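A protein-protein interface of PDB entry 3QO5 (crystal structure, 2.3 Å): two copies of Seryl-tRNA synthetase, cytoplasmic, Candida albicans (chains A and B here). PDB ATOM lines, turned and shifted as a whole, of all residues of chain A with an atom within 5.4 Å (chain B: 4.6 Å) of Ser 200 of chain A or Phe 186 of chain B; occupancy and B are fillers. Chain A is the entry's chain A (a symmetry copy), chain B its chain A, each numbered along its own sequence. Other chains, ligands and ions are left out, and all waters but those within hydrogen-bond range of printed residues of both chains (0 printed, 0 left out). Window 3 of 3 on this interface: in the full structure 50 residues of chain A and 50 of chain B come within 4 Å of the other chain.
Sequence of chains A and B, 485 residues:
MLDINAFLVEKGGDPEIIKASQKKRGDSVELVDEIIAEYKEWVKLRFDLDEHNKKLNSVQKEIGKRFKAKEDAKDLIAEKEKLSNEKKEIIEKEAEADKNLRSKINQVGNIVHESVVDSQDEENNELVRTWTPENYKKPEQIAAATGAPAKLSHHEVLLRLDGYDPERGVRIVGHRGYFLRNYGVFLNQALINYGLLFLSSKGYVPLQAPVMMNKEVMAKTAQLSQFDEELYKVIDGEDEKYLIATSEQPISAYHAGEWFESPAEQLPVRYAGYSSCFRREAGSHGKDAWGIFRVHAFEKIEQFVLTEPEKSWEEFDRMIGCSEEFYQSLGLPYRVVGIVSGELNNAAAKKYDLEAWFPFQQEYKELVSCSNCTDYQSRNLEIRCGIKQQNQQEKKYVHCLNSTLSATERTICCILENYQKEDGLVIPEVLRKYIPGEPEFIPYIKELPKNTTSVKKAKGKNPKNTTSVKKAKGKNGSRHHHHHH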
ATOM      1  N   GLY A 195     -18.619  13.823  20.823  1.00  0.00           N
ATOM      2  CA  GLY A 195     -17.345  13.135  20.931  1.00  0.00           C
ATOM      3  C   GLY A 195     -17.304  11.769  20.243  1.00  0.00           C
ATOM      4  O   GLY A 195     -16.343  11.439  19.539  1.00  0.00           O
ATOM      5  N   LEU A 196     -18.325  10.948  20.471  1.00  0.00           N
ATOM      6  CA  LEU A 196     -18.391   9.627  19.838  1.00  0.00           C
ATOM      7  C   LEU A 196     -18.488   9.772  18.325  1.00  0.00           C
ATOM      8  O   LEU A 196     -17.790   9.081  17.599  1.00  0.00           O
ATOM      9  CB  LEU A 196     -19.608   8.853  20.360  1.00  0.00           C
ATOM     10  CG  LEU A 196     -19.499   8.376  21.802  1.00  0.00           C
ATOM     11  CD1 LEU A 196     -20.840   7.794  22.268  1.00  0.00           C
ATOM     12  CD2 LEU A 196     -18.369   7.315  21.929  1.00  0.00           C
ATOM     13  N   LEU A 197     -19.319  10.705  17.847  1.00  0.00           N
ATOM     14  CA  LEU A 197     -19.429  10.933  16.410  1.00  0.00           C
ATOM     15  C   LEU A 197     -18.102  11.403  15.805  1.00  0.00           C
ATOM     16  O   LEU A 197     -17.724  10.980  14.710  1.00  0.00           O
ATOM     17  CB  LEU A 197     -20.560  11.909  16.086  1.00  0.00           C
ATOM     18  CG  LEU A 197     -20.737  12.153  14.576  1.00  0.00           C
ATOM     19  CD1 LEU A 197     -22.194  12.370  14.218  1.00  0.00           C
ATOM     20  CD2 LEU A 197     -19.928  13.334  14.111  1.00  0.00           C
ATOM     21  N   PHE A 198     -17.393  12.265  16.529  1.00  0.00           N
ATOM     22  CA  PHE A 198     -16.142  12.852  16.040  1.00  0.00           C
ATOM     23  C   PHE A 198     -15.079  11.746  15.883  1.00  0.00           C
ATOM     24  O   PHE A 198     -14.441  11.632  14.847  1.00  0.00           O
ATOM     25  CB  PHE A 198     -15.657  13.925  17.017  1.00  0.00           C
ATOM     26  CG  PHE A 198     -14.334  14.566  16.634  1.00  0.00           C
ATOM     27  CD1 PHE A 198     -14.326  15.695  15.842  1.00  0.00           C
ATOM     28  CD2 PHE A 198     -13.127  14.066  17.087  1.00  0.00           C
ATOM     29  CE1 PHE A 198     -13.123  16.326  15.493  1.00  0.00           C
ATOM     30  CE2 PHE A 198     -11.928  14.683  16.741  1.00  0.00           C
ATOM     31  CZ  PHE A 198     -11.932  15.814  15.938  1.00  0.00           C
ATOM     32  N   LEU A 199     -14.907  10.911  16.901  1.00  0.00           N
ATOM     33  CA  LEU A 199     -13.929   9.832  16.809  1.00  0.00           C
ATOM     34  C   LEU A 199     -14.315   8.733  15.826  1.00  0.00           C
ATOM     35  O   LEU A 199     -13.442   8.201  15.133  1.00  0.00           O
ATOM     36  CB  LEU A 199     -13.631   9.224  18.183  1.00  0.00           C
ATOM     37  CG  LEU A 199     -12.837  10.183  19.082  1.00  0.00           C
ATOM     38  CD1 LEU A 199     -12.556   9.552  20.413  1.00  0.00           C
ATOM     39  CD2 LEU A 199     -11.520  10.558  18.378  1.00  0.00           C
ATOM     40  N   SER A 200     -15.593   8.359  15.775  1.00  0.00           N
ATOM     41  CA  SER A 200     -15.985   7.284  14.875  1.00  0.00           C
ATOM     42  C   SER A 200     -15.770   7.703  13.415  1.00  0.00           C
ATOM     43  O   SER A 200     -15.362   6.900  12.584  1.00  0.00           O
ATOM     44  CB  SER A 200     -17.416   6.786  15.151  1.00  0.00           C
ATOM     45  OG  SER A 200     -18.380   7.731  14.752  1.00  0.00           O
ATOM     46  N   SER A 201     -15.991   8.978  13.117  1.00  0.00           N
ATOM     47  CA  SER A 201     -15.776   9.486  11.766  1.00  0.00           C
ATOM     48  C   SER A 201     -14.291   9.409  11.416  1.00  0.00           C
ATOM     49  O   SER A 201     -13.924   9.472  10.252  1.00  0.00           O
ATOM     50  CB  SER A 201     -16.254  10.938  11.640  1.00  0.00           C
ATOM     51  OG  SER A 201     -15.387  11.837  12.316  1.00  0.00           O
ATOM     52  N   LYS A 202     -13.441   9.316  12.432  1.00  0.00           N
ATOM     53  CA  LYS A 202     -11.997   9.133  12.247  1.00  0.00           C
ATOM     54  C   LYS A 202     -11.573   7.668  12.340  1.00  0.00           C
ATOM     55  O   LYS A 202     -10.394   7.358  12.480  1.00  0.00           O
ATOM     56  CB  LYS A 202     -11.205   9.956  13.246  1.00  0.00           C
ATOM     57  CG  LYS A 202     -11.350  11.432  12.967  1.00  0.00           C
ATOM     58  CD  LYS A 202     -10.554  12.262  13.917  1.00  0.00           C
ATOM     59  CE  LYS A 202     -10.678  13.727  13.556  1.00  0.00           C
ATOM     60  NZ  LYS A 202     -10.319  13.951  12.130  1.00  0.00           N
ATOM     61  N   GLY A 203     -12.549   6.774  12.303  1.00  0.00           N
ATOM     62  CA  GLY A 203     -12.269   5.354  12.305  1.00  0.00           C
ATOM     63  C   GLY A 203     -12.147   4.717  13.678  1.00  0.00           C
ATOM     64  O   GLY A 203     -11.697   3.576  13.787  1.00  0.00           O
ATOM     65  N   TYR A 204     -12.457   5.455  14.737  1.00  0.00           N
ATOM     66  CA  TYR A 204     -12.455   4.825  16.048  1.00  0.00           C
ATOM     67  C   TYR A 204     -13.727   3.972  16.241  1.00  0.00           C
ATOM     68  O   TYR A 204     -14.816   4.345  15.782  1.00  0.00           O
ATOM     69  CB  TYR A 204     -12.429   5.876  17.135  1.00  0.00           C
ATOM     70  CG  TYR A 204     -11.089   6.544  17.282  1.00  0.00           C
ATOM     71  CD1 TYR A 204     -10.384   6.462  18.470  1.00  0.00           C
ATOM     72  CD2 TYR A 204     -10.561   7.326  16.255  1.00  0.00           C
ATOM     73  CE1 TYR A 204      -9.169   7.093  18.622  1.00  0.00           C
ATOM     74  CE2 TYR A 204      -9.366   7.962  16.401  1.00  0.00           C
ATOM     75  CZ  TYR A 204      -8.660   7.835  17.584  1.00  0.00           C
ATOM     76  OH  TYR A 204      -7.438   8.465  17.734  1.00  0.00           O
ATOM     77  N   PRO A 206     -16.634   2.909  18.621  1.00  0.00           N
ATOM     78  CA  PRO A 206     -17.237   3.260  19.914  1.00  0.00           C
ATOM     79  C   PRO A 206     -17.285   2.038  20.818  1.00  0.00           C
ATOM     80  O   PRO A 206     -17.657   0.933  20.393  1.00  0.00           O
ATOM     81  CB  PRO A 206     -18.663   3.681  19.531  1.00  0.00           C
ATOM     82  CG  PRO A 206     -18.539   4.151  18.089  1.00  0.00           C
ATOM     83  CD  PRO A 206     -17.522   3.215  17.483  1.00  0.00           C
ATOM     84  N   ALA A 272     -12.956   4.453  20.607  1.00  0.00           N
ATOM     85  CA  ALA A 272     -13.533   5.619  21.225  1.00  0.00           C
ATOM     86  C   ALA A 272     -14.196   5.160  22.503  1.00  0.00           C
ATOM     87  O   ALA A 272     -15.371   4.787  22.494  1.00  0.00           O
ATOM     88  CB  ALA A 272     -14.537   6.260  20.290  1.00  0.00           C
ATOM     89  N   ASN B 182     -19.947  -0.200  19.128  1.00  0.00           N
ATOM     90  CA  ASN B 182     -20.532   0.402  17.959  1.00  0.00           C
ATOM     91  C   ASN B 182     -21.999   0.794  18.090  1.00  0.00           C
ATOM     92  O   ASN B 182     -22.338   1.682  18.868  1.00  0.00           O
ATOM     93  CB  ASN B 182     -20.335  -0.516  16.765  1.00  0.00           C
ATOM     94  CG  ASN B 182     -19.594   0.165  15.671  1.00  0.00           C
ATOM     95  OD1 ASN B 182     -18.564  -0.333  15.216  1.00  0.00           O
ATOM     96  ND2 ASN B 182     -20.076   1.350  15.264  1.00  0.00           N
ATOM     97  N   TYR B 183     -22.858   0.158  17.293  1.00  0.00           N
ATOM     98  CA  TYR B 183     -24.266   0.523  17.291  1.00  0.00           C
ATOM     99  C   TYR B 183     -24.941   0.231  18.619  1.00  0.00           C
ATOM    100  O   TYR B 183     -25.978   0.808  18.923  1.00  0.00           O
ATOM    101  CB  TYR B 183     -25.008  -0.090  16.103  1.00  0.00           C
ATOM    102  CG  TYR B 183     -24.659   0.609  14.810  1.00  0.00           C
ATOM    103  CD1 TYR B 183     -25.097   1.899  14.559  1.00  0.00           C
ATOM    104  CD2 TYR B 183     -23.854  -0.012  13.857  1.00  0.00           C
ATOM    105  CE1 TYR B 183     -24.762   2.554  13.377  1.00  0.00           C
ATOM    106  CE2 TYR B 183     -23.524   0.623  12.680  1.00  0.00           C
ATOM    107  CZ  TYR B 183     -23.977   1.909  12.443  1.00  0.00           C
ATOM    108  OH  TYR B 183     -23.646   2.528  11.260  1.00  0.00           O
ATOM    109  N   GLY B 184     -24.359  -0.676  19.396  1.00  0.00           N
ATOM    110  CA  GLY B 184     -24.836  -0.888  20.749  1.00  0.00           C
ATOM    111  C   GLY B 184     -24.714   0.395  21.546  1.00  0.00           C
ATOM    112  O   GLY B 184     -25.614   0.776  22.310  1.00  0.00           O
ATOM    113  N   VAL B 185     -23.598   1.088  21.336  1.00  0.00           N
ATOM    114  CA  VAL B 185     -23.358   2.338  22.036  1.00  0.00           C
ATOM    115  C   VAL B 185     -24.326   3.386  21.515  1.00  0.00           C
ATOM    116  O   VAL B 185     -25.027   4.049  22.285  1.00  0.00           O
ATOM    117  CB  VAL B 185     -21.916   2.807  21.838  1.00  0.00           C
ATOM    118  CG1 VAL B 185     -21.700   4.134  22.573  1.00  0.00           C
ATOM    119  CG2 VAL B 185     -20.960   1.766  22.394  1.00  0.00           C
ATOM    120  N   PHE B 186     -24.407   3.481  20.197  1.00  0.00           N
ATOM    121  CA  PHE B 186     -25.240   4.501  19.578  1.00  0.00           C
ATOM    122  C   PHE B 186     -26.717   4.299  19.920  1.00  0.00           C
ATOM    123  O   PHE B 186     -27.438   5.277  20.157  1.00  0.00           O
ATOM    124  CB  PHE B 186     -25.044   4.497  18.064  1.00  0.00           C
ATOM    125  CG  PHE B 186     -23.684   5.008  17.630  1.00  0.00           C
ATOM    126  CD1 PHE B 186     -23.096   6.093  18.271  1.00  0.00           C
ATOM    127  CD2 PHE B 186     -23.006   4.409  16.575  1.00  0.00           C
ATOM    128  CE1 PHE B 186     -21.847   6.561  17.877  1.00  0.00           C
ATOM    129  CE2 PHE B 186     -21.757   4.880  16.167  1.00  0.00           C
ATOM    130  CZ  PHE B 186     -21.176   5.949  16.820  1.00  0.00           C
ATOM    131  N   LEU B 187     -27.164   3.035  19.974  1.00  0.00           N
ATOM    132  CA  LEU B 187     -28.568   2.747  20.329  1.00  0.00           C
ATOM    133  C   LEU B 187     -28.851   3.106  21.785  1.00  0.00           C
ATOM    134  O   LEU B 187     -29.896   3.665  22.090  1.00  0.00           O
ATOM    135  CB  LEU B 187     -28.919   1.280  20.096  1.00  0.00           C
ATOM    136  CG  LEU B 187     -29.264   0.923  18.647  1.00  0.00           C
ATOM    137  CD1 LEU B 187     -29.211  -0.598  18.423  1.00  0.00           C
ATOM    138  CD2 LEU B 187     -30.654   1.484  18.242  1.00  0.00           C
ATOM    139  N   ASN B 188     -27.921   2.788  22.682  1.00  0.00           N
ATOM    140  CA  ASN B 188     -28.105   3.121  24.093  1.00  0.00           C
ATOM    141  C   ASN B 188     -28.208   4.648  24.294  1.00  0.00           C
ATOM    142  O   ASN B 188     -29.110   5.143  24.971  1.00  0.00           O
ATOM    143  CB  ASN B 188     -26.959   2.572  24.928  1.00  0.00           C
ATOM    144  CG  ASN B 188     -27.332   2.405  26.369  1.00  0.00           C
ATOM    145  OD1 ASN B 188     -28.357   1.780  26.702  1.00  0.00           O
ATOM    146  ND2 ASN B 188     -26.540   3.018  27.252  1.00  0.00           N
ATOM    147  N   GLN B 189     -27.266   5.392  23.713  1.00  0.00           N
ATOM    148  CA  GLN B 189     -27.305   6.862  23.760  1.00  0.00           C
ATOM    149  C   GLN B 189     -28.561   7.437  23.109  1.00  0.00           C
ATOM    150  O   GLN B 189     -29.189   8.374  23.624  1.00  0.00           O
ATOM    151  CB  GLN B 189     -26.055   7.473  23.117  1.00  0.00           C
ATOM    152  CG  GLN B 189     -24.780   7.293  23.959  1.00  0.00           C
ATOM    153  CD  GLN B 189     -24.830   8.026  25.273  1.00  0.00           C
ATOM    154  OE1 GLN B 189     -24.599   7.422  26.317  1.00  0.00           O
ATOM    155  NE2 GLN B 189     -25.148   9.324  25.247  1.00  0.00           N
ATOM    156  N   ALA B 190     -28.956   6.840  21.987  1.00  0.00           N
ATOM    157  CA  ALA B 190     -30.170   7.290  21.324  1.00  0.00           C
ATOM    158  C   ALA B 190     -31.366   7.241  22.265  1.00  0.00           C
ATOM    159  O   ALA B 190     -32.143   8.194  22.340  1.00  0.00           O
ATOM    160  CB  ALA B 190     -30.447   6.490  20.036  1.00  0.00           C
ATOM    161  N   ILE B 435     -28.358   8.850  15.656  1.00  0.00           N
ATOM    162  CA  ILE B 435     -27.299   7.932  15.329  1.00  0.00           C
ATOM    163  C   ILE B 435     -26.524   8.419  14.125  1.00  0.00           C
ATOM    164  O   ILE B 435     -27.100   8.799  13.108  1.00  0.00           O
ATOM    165  CB  ILE B 435     -27.887   6.548  15.028  1.00  0.00           C
ATOM    166  CG1 ILE B 435     -28.512   5.983  16.307  1.00  0.00           C
ATOM    167  CG2 ILE B 435     -26.814   5.617  14.514  1.00  0.00           C
ATOM    168  CD1 ILE B 435     -29.428   4.786  16.080  1.00  0.00           C
ATOM    169  N   PRO B 436     -25.196   8.423  14.244  1.00  0.00           N
ATOM    170  CA  PRO B 436     -24.432   8.957  13.115  1.00  0.00           C
ATOM    171  C   PRO B 436     -24.784   8.239  11.819  1.00  0.00           C
ATOM    172  O   PRO B 436     -24.846   7.013  11.785  1.00  0.00           O
ATOM    173  CB  PRO B 436     -22.982   8.642  13.497  1.00  0.00           C
ATOM    174  CG  PRO B 436     -23.004   8.602  15.018  1.00  0.00           C
ATOM    175  CD  PRO B 436     -24.344   8.034  15.379  1.00  0.00           C
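No position is printed for both chains.
Of the 6 pairs that touch across the chains among the printed residues, none has its exchanged pair printed and touching as well.
O of Leu 197 of chain A is in hydrogen-bond range of OG of Ser 200 of chain A.
OG of Ser 201 of chain A sits close to O of Leu 197 of chain A (3.5 Å).
The backbone carbonyl oxygen (O) of Leu 196 of chain A lies within hydrogen-bond range of the side-chain hydroxyl (OG) of Ser 200 of chain A (3.2 Å).
Printed residues of chain B within 4 Å of Leu 196 of chain A: Val 185.
Printed residues of chain B within 4 Å of Leu 197 of chain A: Pro 436.
Of chain B, only Phe 186 (3.9 Å) comes within 4 Å of Ser 200 of chain A.
Of the printed residues of chain B, Pro 206 of chain A touches Asn 182 (2.9 Å), Val 185 (3.95 Å) and Phe 186 (3.4 Å).
Of the printed residues of chain A, Asn 182 of chain B touches Pro 206 (2.9 Å).
Gly 184 of chain B touches none of the printed residues of chain A.
Printed residues of chain A within 4 Å of Val 185 of chain B: Leu 196 and Pro 206.
Phe 186 of chain B touches just these residues of chain A: Ser 200 and Pro 206.
The nearest residue of chain A that does not touch Phe 186 of chain B is Leu 196 of chain A (4.1 Å).
N of Asn 182 of chain B sits at hydrogen-bond distance from O of Pro 206 of chain A.
Printed residues of chain A that touch a printed residue of chain B: Leu 196, Leu 197, Ser 200 and Pro 206.
Hydrophobic or aromatic side chains of chain A within 4 Å of the printed part of chain B: Leu 196, Leu 197 and Pro 206.
Printed residues of chain B that touch a printed residue of chain A: Asn 182, Val 185, Phe 186 and Pro 436.
Among the printed residues, 6 pairs touch across the chains.
Among the printed residues, no Asp or Glu carboxylate lies within 4 Å of a Lys or Arg side-chain nitrogen of the other chain.
Among the printed residues, merely in contact across the chains: Leu 196 of chain A with Val 185 of chain B (3.8 Å), Leu 197 of chain A with Pro 436 of chain B (3.9 Å), Ser 200 of chain A with Phe 186 of chain B (3.9 Å), Pro 206 of chain A with Val 185 of chain B (3.95 Å) and Pro 206 of chain A with Phe 186 of chain B (3.4 Å).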
